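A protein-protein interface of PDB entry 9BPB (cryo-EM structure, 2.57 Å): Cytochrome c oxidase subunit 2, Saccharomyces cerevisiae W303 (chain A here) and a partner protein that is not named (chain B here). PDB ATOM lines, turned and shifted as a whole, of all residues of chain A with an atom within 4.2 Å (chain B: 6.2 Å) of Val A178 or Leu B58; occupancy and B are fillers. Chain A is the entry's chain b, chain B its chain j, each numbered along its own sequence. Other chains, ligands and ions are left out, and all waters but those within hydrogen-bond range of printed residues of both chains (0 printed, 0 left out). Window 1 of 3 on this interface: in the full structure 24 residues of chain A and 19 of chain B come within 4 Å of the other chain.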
ATOM      1  N   THR A 116       6.747 -26.187  22.419  1.00  0.00           N
ATOM      2  CA  THR A 116       7.052 -25.189  23.436  1.00  0.00           C
ATOM      3  C   THR A 116       8.019 -25.757  24.468  1.00  0.00           C
ATOM      4  O   THR A 116       7.886 -26.911  24.889  1.00  0.00           O
ATOM      5  CB  THR A 116       5.768 -24.714  24.136  1.00  0.00           C
ATOM      6  OG1 THR A 116       4.862 -24.176  23.165  1.00  0.00           O
ATOM      7  CG2 THR A 116       6.078 -23.639  25.168  1.00  0.00           C
ATOM      8  N   ILE A 117       8.988 -24.939  24.879  1.00  0.00           N
ATOM      9  CA  ILE A 117       9.977 -25.311  25.883  1.00  0.00           C
ATOM     10  C   ILE A 117       9.911 -24.318  27.033  1.00  0.00           C
ATOM     11  O   ILE A 117       9.922 -23.102  26.817  1.00  0.00           O
ATOM     12  CB  ILE A 117      11.410 -25.355  25.310  1.00  0.00           C
ATOM     13  CG1 ILE A 117      11.556 -26.464  24.270  1.00  0.00           C
ATOM     14  CG2 ILE A 117      12.431 -25.521  26.423  1.00  0.00           C
ATOM     15  CD1 ILE A 117      11.313 -25.992  22.874  1.00  0.00           C
ATOM     16  N   LYS A 118       9.850 -24.840  28.251  1.00  0.00           N
ATOM     17  CA  LYS A 118       9.928 -24.035  29.460  1.00  0.00           C
ATOM     18  C   LYS A 118      11.355 -24.026  29.997  1.00  0.00           C
ATOM     19  O   LYS A 118      12.066 -25.032  29.956  1.00  0.00           O
ATOM     20  CB  LYS A 118       8.974 -24.566  30.527  1.00  0.00           C
ATOM     21  CG  LYS A 118       7.569 -24.806  30.034  1.00  0.00           C
ATOM     22  CD  LYS A 118       6.609 -24.840  31.198  1.00  0.00           C
ATOM     23  CE  LYS A 118       6.906 -26.023  32.098  1.00  0.00           C
ATOM     24  NZ  LYS A 118       6.415 -27.310  31.541  1.00  0.00           N
ATOM     25  N   ALA A 119      11.766 -22.872  30.516  1.00  0.00           N
ATOM     26  CA  ALA A 119      13.129 -22.713  31.019  1.00  0.00           C
ATOM     27  C   ALA A 119      13.050 -22.044  32.388  1.00  0.00           C
ATOM     28  O   ALA A 119      12.783 -20.842  32.480  1.00  0.00           O
ATOM     29  CB  ALA A 119      13.982 -21.907  30.051  1.00  0.00           C
ATOM     30  N   SER A 131       7.117 -29.425  28.041  1.00  0.00           N
ATOM     31  CA  SER A 131       5.736 -29.676  28.428  1.00  0.00           C
ATOM     32  C   SER A 131       4.940 -30.390  27.343  1.00  0.00           C
ATOM     33  O   SER A 131       3.874 -30.940  27.638  1.00  0.00           O
ATOM     34  CB  SER A 131       5.072 -28.353  28.792  1.00  0.00           C
ATOM     35  OG  SER A 131       4.880 -27.545  27.643  1.00  0.00           O
ATOM     36  N   PHE A 177       9.268 -20.273  23.673  1.00  0.00           N
ATOM     37  CA  PHE A 177       9.933 -20.365  24.965  1.00  0.00           C
ATOM     38  C   PHE A 177       9.104 -19.657  26.023  1.00  0.00           C
ATOM     39  O   PHE A 177       8.622 -18.547  25.802  1.00  0.00           O
ATOM     40  CB  PHE A 177      11.330 -19.746  24.914  1.00  0.00           C
ATOM     41  CG  PHE A 177      12.336 -20.573  24.168  1.00  0.00           C
ATOM     42  CD1 PHE A 177      12.444 -21.933  24.401  1.00  0.00           C
ATOM     43  CD2 PHE A 177      13.184 -19.987  23.244  1.00  0.00           C
ATOM     44  CE1 PHE A 177      13.370 -22.694  23.720  1.00  0.00           C
ATOM     45  CE2 PHE A 177      14.112 -20.744  22.561  1.00  0.00           C
ATOM     46  CZ  PHE A 177      14.206 -22.098  22.802  1.00  0.00           C
ATOM     47  N   VAL A 178       8.936 -20.304  27.175  1.00  0.00           N
ATOM     48  CA  VAL A 178       8.260 -19.717  28.325  1.00  0.00           C
ATOM     49  C   VAL A 178       9.191 -19.852  29.520  1.00  0.00           C
ATOM     50  O   VAL A 178       9.547 -20.972  29.903  1.00  0.00           O
ATOM     51  CB  VAL A 178       6.910 -20.392  28.613  1.00  0.00           C
ATOM     52  CG1 VAL A 178       6.278 -19.800  29.857  1.00  0.00           C
ATOM     53  CG2 VAL A 178       5.980 -20.252  27.421  1.00  0.00           C
ATOM     54  N   VAL A 179       9.585 -18.728  30.108  1.00  0.00           N
ATOM     55  CA  VAL A 179      10.601 -18.737  31.151  1.00  0.00           C
ATOM     56  C   VAL A 179      10.021 -18.174  32.440  1.00  0.00           C
ATOM     57  O   VAL A 179       9.115 -17.335  32.428  1.00  0.00           O
ATOM     58  CB  VAL A 179      11.856 -17.938  30.744  1.00  0.00           C
ATOM     59  CG1 VAL A 179      12.483 -18.527  29.491  1.00  0.00           C
ATOM     60  CG2 VAL A 179      11.512 -16.478  30.566  1.00  0.00           C
ATOM     61  N   LEU A 204       5.412 -15.544  33.665  1.00  0.00           N
ATOM     62  CA  LEU A 204       5.742 -16.406  32.534  1.00  0.00           C
ATOM     63  C   LEU A 204       5.747 -15.563  31.264  1.00  0.00           C
ATOM     64  O   LEU A 204       4.696 -15.353  30.651  1.00  0.00           O
ATOM     65  CB  LEU A 204       4.750 -17.562  32.414  1.00  0.00           C
ATOM     66  CG  LEU A 204       4.576 -18.476  33.624  1.00  0.00           C
ATOM     67  CD1 LEU A 204       3.312 -19.304  33.485  1.00  0.00           C
ATOM     68  CD2 LEU A 204       5.784 -19.377  33.776  1.00  0.00           C
ATOM     69  N   ASN A 205       6.925 -15.090  30.868  1.00  0.00           N
ATOM     70  CA  ASN A 205       7.107 -14.327  29.642  1.00  0.00           C
ATOM     71  C   ASN A 205       7.563 -15.256  28.524  1.00  0.00           C
ATOM     72  O   ASN A 205       8.254 -16.248  28.767  1.00  0.00           O
ATOM     73  CB  ASN A 205       8.124 -13.203  29.842  1.00  0.00           C
ATOM     74  CG  ASN A 205       7.892 -12.435  31.125  1.00  0.00           C
ATOM     75  OD1 ASN A 205       6.828 -11.854  31.330  1.00  0.00           O
ATOM     76  ND2 ASN A 205       8.883 -12.438  32.004  1.00  0.00           N
ATOM     77  N   GLN A 206       7.173 -14.930  27.291  1.00  0.00           N
ATOM     78  CA  GLN A 206       7.369 -15.836  26.170  1.00  0.00           C
ATOM     79  C   GLN A 206       7.961 -15.120  24.963  1.00  0.00           C
ATOM     80  O   GLN A 206       7.796 -13.909  24.791  1.00  0.00           O
ATOM     81  CB  GLN A 206       6.052 -16.511  25.766  1.00  0.00           C
ATOM     82  CG  GLN A 206       5.183 -15.683  24.839  1.00  0.00           C
ATOM     83  CD  GLN A 206       4.017 -16.469  24.282  1.00  0.00           C
ATOM     84  OE1 GLN A 206       3.786 -17.610  24.670  1.00  0.00           O
ATOM     85  NE2 GLN A 206       3.276 -15.860  23.366  1.00  0.00           N
ATOM     86  N   VAL B  12      -0.014 -25.468  21.437  1.00  0.00           N
ATOM     87  CA  VAL B  12      -1.163 -24.598  21.647  1.00  0.00           C
ATOM     88  C   VAL B  12      -1.126 -23.434  20.663  1.00  0.00           C
ATOM     89  O   VAL B  12      -0.062 -22.883  20.350  1.00  0.00           O
ATOM     90  CB  VAL B  12      -1.183 -24.100  23.105  1.00  0.00           C
ATOM     91  CG1 VAL B  12      -2.393 -23.216  23.361  1.00  0.00           C
ATOM     92  CG2 VAL B  12      -1.157 -25.279  24.065  1.00  0.00           C
ATOM     93  N   GLN B  23       1.999 -14.356  30.261  1.00  0.00           N
ATOM     94  CA  GLN B  23       1.107 -15.495  30.077  1.00  0.00           C
ATOM     95  C   GLN B  23       0.722 -16.162  31.393  1.00  0.00           C
ATOM     96  O   GLN B  23       0.325 -17.330  31.390  1.00  0.00           O
ATOM     97  CB  GLN B  23       1.744 -16.526  29.141  1.00  0.00           C
ATOM     98  CG  GLN B  23       1.988 -16.020  27.729  1.00  0.00           C
ATOM     99  CD  GLN B  23       0.786 -16.199  26.828  1.00  0.00           C
ATOM    100  OE1 GLN B  23      -0.157 -16.910  27.164  1.00  0.00           O
ATOM    101  NE2 GLN B  23       0.813 -15.546  25.674  1.00  0.00           N
ATOM    102  N   HIS B  26      -3.038 -16.987  31.386  1.00  0.00           N
ATOM    103  CA  HIS B  26      -3.390 -18.030  30.428  1.00  0.00           C
ATOM    104  C   HIS B  26      -3.185 -19.417  31.029  1.00  0.00           C
ATOM    105  O   HIS B  26      -3.996 -20.324  30.810  1.00  0.00           O
ATOM    106  CB  HIS B  26      -2.563 -17.858  29.154  1.00  0.00           C
ATOM    107  CG  HIS B  26      -3.160 -18.514  27.949  1.00  0.00           C
ATOM    108  ND1 HIS B  26      -2.535 -18.514  26.720  1.00  0.00           N
ATOM    109  CD2 HIS B  26      -4.321 -19.188  27.782  1.00  0.00           C
ATOM    110  CE1 HIS B  26      -3.286 -19.164  25.848  1.00  0.00           C
ATOM    111  NE2 HIS B  26      -4.375 -19.581  26.466  1.00  0.00           N
ATOM    112  N   CYS B  27      -2.098 -19.598  31.782  1.00  0.00           N
ATOM    113  CA  CYS B  27      -1.902 -20.832  32.538  1.00  0.00           C
ATOM    114  C   CYS B  27      -2.974 -21.014  33.605  1.00  0.00           C
ATOM    115  O   CYS B  27      -3.551 -22.100  33.732  1.00  0.00           O
ATOM    116  CB  CYS B  27      -0.518 -20.825  33.182  1.00  0.00           C
ATOM    117  SG  CYS B  27      -0.206 -22.215  34.279  1.00  0.00           S
ATOM    118  N   SER B  30      -6.702 -21.958  32.501  1.00  0.00           N
ATOM    119  CA  SER B  30      -6.864 -23.336  32.048  1.00  0.00           C
ATOM    120  C   SER B  30      -7.006 -24.293  33.225  1.00  0.00           C
ATOM    121  O   SER B  30      -7.766 -25.266  33.154  1.00  0.00           O
ATOM    122  CB  SER B  30      -5.685 -23.735  31.163  1.00  0.00           C
ATOM    123  OG  SER B  30      -5.466 -22.771  30.150  1.00  0.00           O
ATOM    124  N   THR B  54      -3.502 -27.988  27.935  1.00  0.00           N
ATOM    125  CA  THR B  54      -3.096 -26.591  27.882  1.00  0.00           C
ATOM    126  C   THR B  54      -2.411 -26.122  29.161  1.00  0.00           C
ATOM    127  O   THR B  54      -1.546 -25.240  29.092  1.00  0.00           O
ATOM    128  CB  THR B  54      -4.311 -25.706  27.583  1.00  0.00           C
ATOM    129  OG1 THR B  54      -4.979 -26.199  26.414  1.00  0.00           O
ATOM    130  CG2 THR B  54      -3.893 -24.269  27.332  1.00  0.00           C
ATOM    131  N   TYR B  55      -2.754 -26.676  30.331  1.00  0.00           N
ATOM    132  CA  TYR B  55      -2.002 -26.284  31.518  1.00  0.00           C
ATOM    133  C   TYR B  55      -0.872 -27.255  31.824  1.00  0.00           C
ATOM    134  O   TYR B  55       0.114 -26.865  32.455  1.00  0.00           O
ATOM    135  CB  TYR B  55      -2.887 -26.153  32.768  1.00  0.00           C
ATOM    136  CG  TYR B  55      -3.556 -27.410  33.285  1.00  0.00           C
ATOM    137  CD1 TYR B  55      -4.807 -27.803  32.853  1.00  0.00           C
ATOM    138  CD2 TYR B  55      -2.924 -28.190  34.243  1.00  0.00           C
ATOM    139  CE1 TYR B  55      -5.407 -28.951  33.360  1.00  0.00           C
ATOM    140  CE2 TYR B  55      -3.508 -29.328  34.742  1.00  0.00           C
ATOM    141  CZ  TYR B  55      -4.748 -29.706  34.302  1.00  0.00           C
ATOM    142  OH  TYR B  55      -5.320 -30.850  34.811  1.00  0.00           O
ATOM    143  N   ASN B  56      -0.996 -28.517  31.410  1.00  0.00           N
ATOM    144  CA  ASN B  56       0.162 -29.403  31.441  1.00  0.00           C
ATOM    145  C   ASN B  56       1.273 -28.849  30.559  1.00  0.00           C
ATOM    146  O   ASN B  56       2.458 -29.103  30.798  1.00  0.00           O
ATOM    147  CB  ASN B  56      -0.235 -30.809  30.998  1.00  0.00           C
ATOM    148  CG  ASN B  56      -0.913 -31.592  32.100  1.00  0.00           C
ATOM    149  OD1 ASN B  56      -0.295 -31.926  33.109  1.00  0.00           O
ATOM    150  ND2 ASN B  56      -2.196 -31.878  31.917  1.00  0.00           N
ATOM    151  N   ALA B  57       0.900 -28.100  29.527  1.00  0.00           N
ATOM    152  CA  ALA B  57       1.830 -27.257  28.803  1.00  0.00           C
ATOM    153  C   ALA B  57       1.836 -25.853  29.403  1.00  0.00           C
ATOM    154  O   ALA B  57       0.949 -25.474  30.174  1.00  0.00           O
ATOM    155  CB  ALA B  57       1.469 -27.207  27.319  1.00  0.00           C
ATOM    156  N   LEU B  58       2.881 -25.091  29.080  1.00  0.00           N
ATOM    157  CA  LEU B  58       2.916 -23.660  29.357  1.00  0.00           C
ATOM    158  C   LEU B  58       2.990 -23.348  30.852  1.00  0.00           C
ATOM    159  O   LEU B  58       3.120 -22.181  31.234  1.00  0.00           O
ATOM    160  CB  LEU B  58       1.692 -22.988  28.719  1.00  0.00           C
ATOM    161  CG  LEU B  58       1.477 -21.472  28.760  1.00  0.00           C
ATOM    162  CD1 LEU B  58       2.350 -20.761  27.741  1.00  0.00           C
ATOM    163  CD2 LEU B  58       0.013 -21.149  28.531  1.00  0.00           C
ATOM    164  N   CYS B  59       2.944 -24.367  31.708  1.00  0.00           N
ATOM    165  CA  CYS B  59       2.926 -24.144  33.146  1.00  0.00           C
ATOM    166  C   CYS B  59       4.049 -24.911  33.828  1.00  0.00           C
ATOM    167  O   CYS B  59       4.226 -26.107  33.558  1.00  0.00           O
ATOM    168  CB  CYS B  59       1.585 -24.568  33.748  1.00  0.00           C
ATOM    169  SG  CYS B  59       0.151 -23.762  33.023  1.00  0.00           S
ATOM    170  N   PRO B  60       4.806 -24.279  34.727  1.00  0.00           N
ATOM    171  CA  PRO B  60       5.860 -25.002  35.447  1.00  0.00           C
ATOM    172  C   PRO B  60       5.278 -26.130  36.284  1.00  0.00           C
ATOM    173  O   PRO B  60       4.142 -26.059  36.756  1.00  0.00           O
ATOM    174  CB  PRO B  60       6.497 -23.921  36.328  1.00  0.00           C
ATOM    175  CG  PRO B  60       6.101 -22.625  35.694  1.00  0.00           C
ATOM    176  CD  PRO B  60       4.745 -22.862  35.115  1.00  0.00           C
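Among the printed residues, merely in contact across the chains: Ser A131 with Ala B57 (3.3 Å), Ser A131 with Asn B56 (3.4 Å), Lys A118 with Pro B60 (3.7 Å), Leu A204 with Leu B58 (3.7 Å), Val A178 with Leu B58 (3.7 Å), Leu A204 with Pro B60 (3.8 Å) and Lys A118 with Leu B58 (3.9 Å).
Of chain B, only Leu B58 comes within 4 Å of Val A178. Of chain A, only Lys A118, Ser A131, Val A178 and Leu A204 come within 4 Å of Leu B58. Of the printed residues of chain A, Asn B56 touches Ser A131 (3.4 Å). Printed residues of chain A within 4 Å of Pro B60: Lys A118 and Leu A204. Of the printed residues of chain B, Leu A204 touches Gln B23 (2.9 Å), Leu B58 (3.7 Å) and Pro B60 (3.8 Å). Of the printed residues of chain A, Gln B23 touches Leu A204 (2.9 Å) and Gln A206 (3.4 Å). Ser B30 touches none of the printed residues of chain A. The nearest residue of chain B that does not touch Val A178 is Gln B23 (5.6 Å). The nearest printed residue of chain A that does not touch Leu B58 is Gln A206 (4.6 Å).
N of Val A178 sits at hydrogen-bond distance from O of Ile A117, 3.0 Å away. The backbone NH (N) of Ala A119 is in hydrogen-bond range of the backbone carbonyl oxygen (O) of Val A178 (3.0 Å). The side-chain amide oxygen (OE1) of Gln B23 is in hydrogen-bond range of a ring nitrogen (ND1) of His B26. SG of Cys B27 forms a disulfide with SG of Cys B59, at 2.0 Å.
NZ of Lys A118 sits close to O of Cys B59. OG of Ser A131 is in hydrogen-bond range of N of Leu B58, 3.5 Å away. The backbone carbonyl oxygen of Leu A204 sits at hydrogen-bond distance from the backbone NH of Gln B23, 2.9 Å away. The side-chain amide nitrogen (NE2) of Gln A206 sits close to the side-chain amide nitrogen (NE2) of Gln B23.
Of the 12 printed residues of chain B, 6 touch a printed residue of chain A. Hydrophobic or aromatic side chains of chain B that line the printed part of chain A: Ala B57, Leu B58 and Pro B60. Of the 11 printed residues of chain A, 5 touch a printed residue of chain B. Along chain A the printed residues that touch a printed residue of chain B span positions 118 to 206. Among the printed residues, no Asp or Glu carboxylate lies within 4 Å of a Lys or Arg side-chain nitrogen of the other chain.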
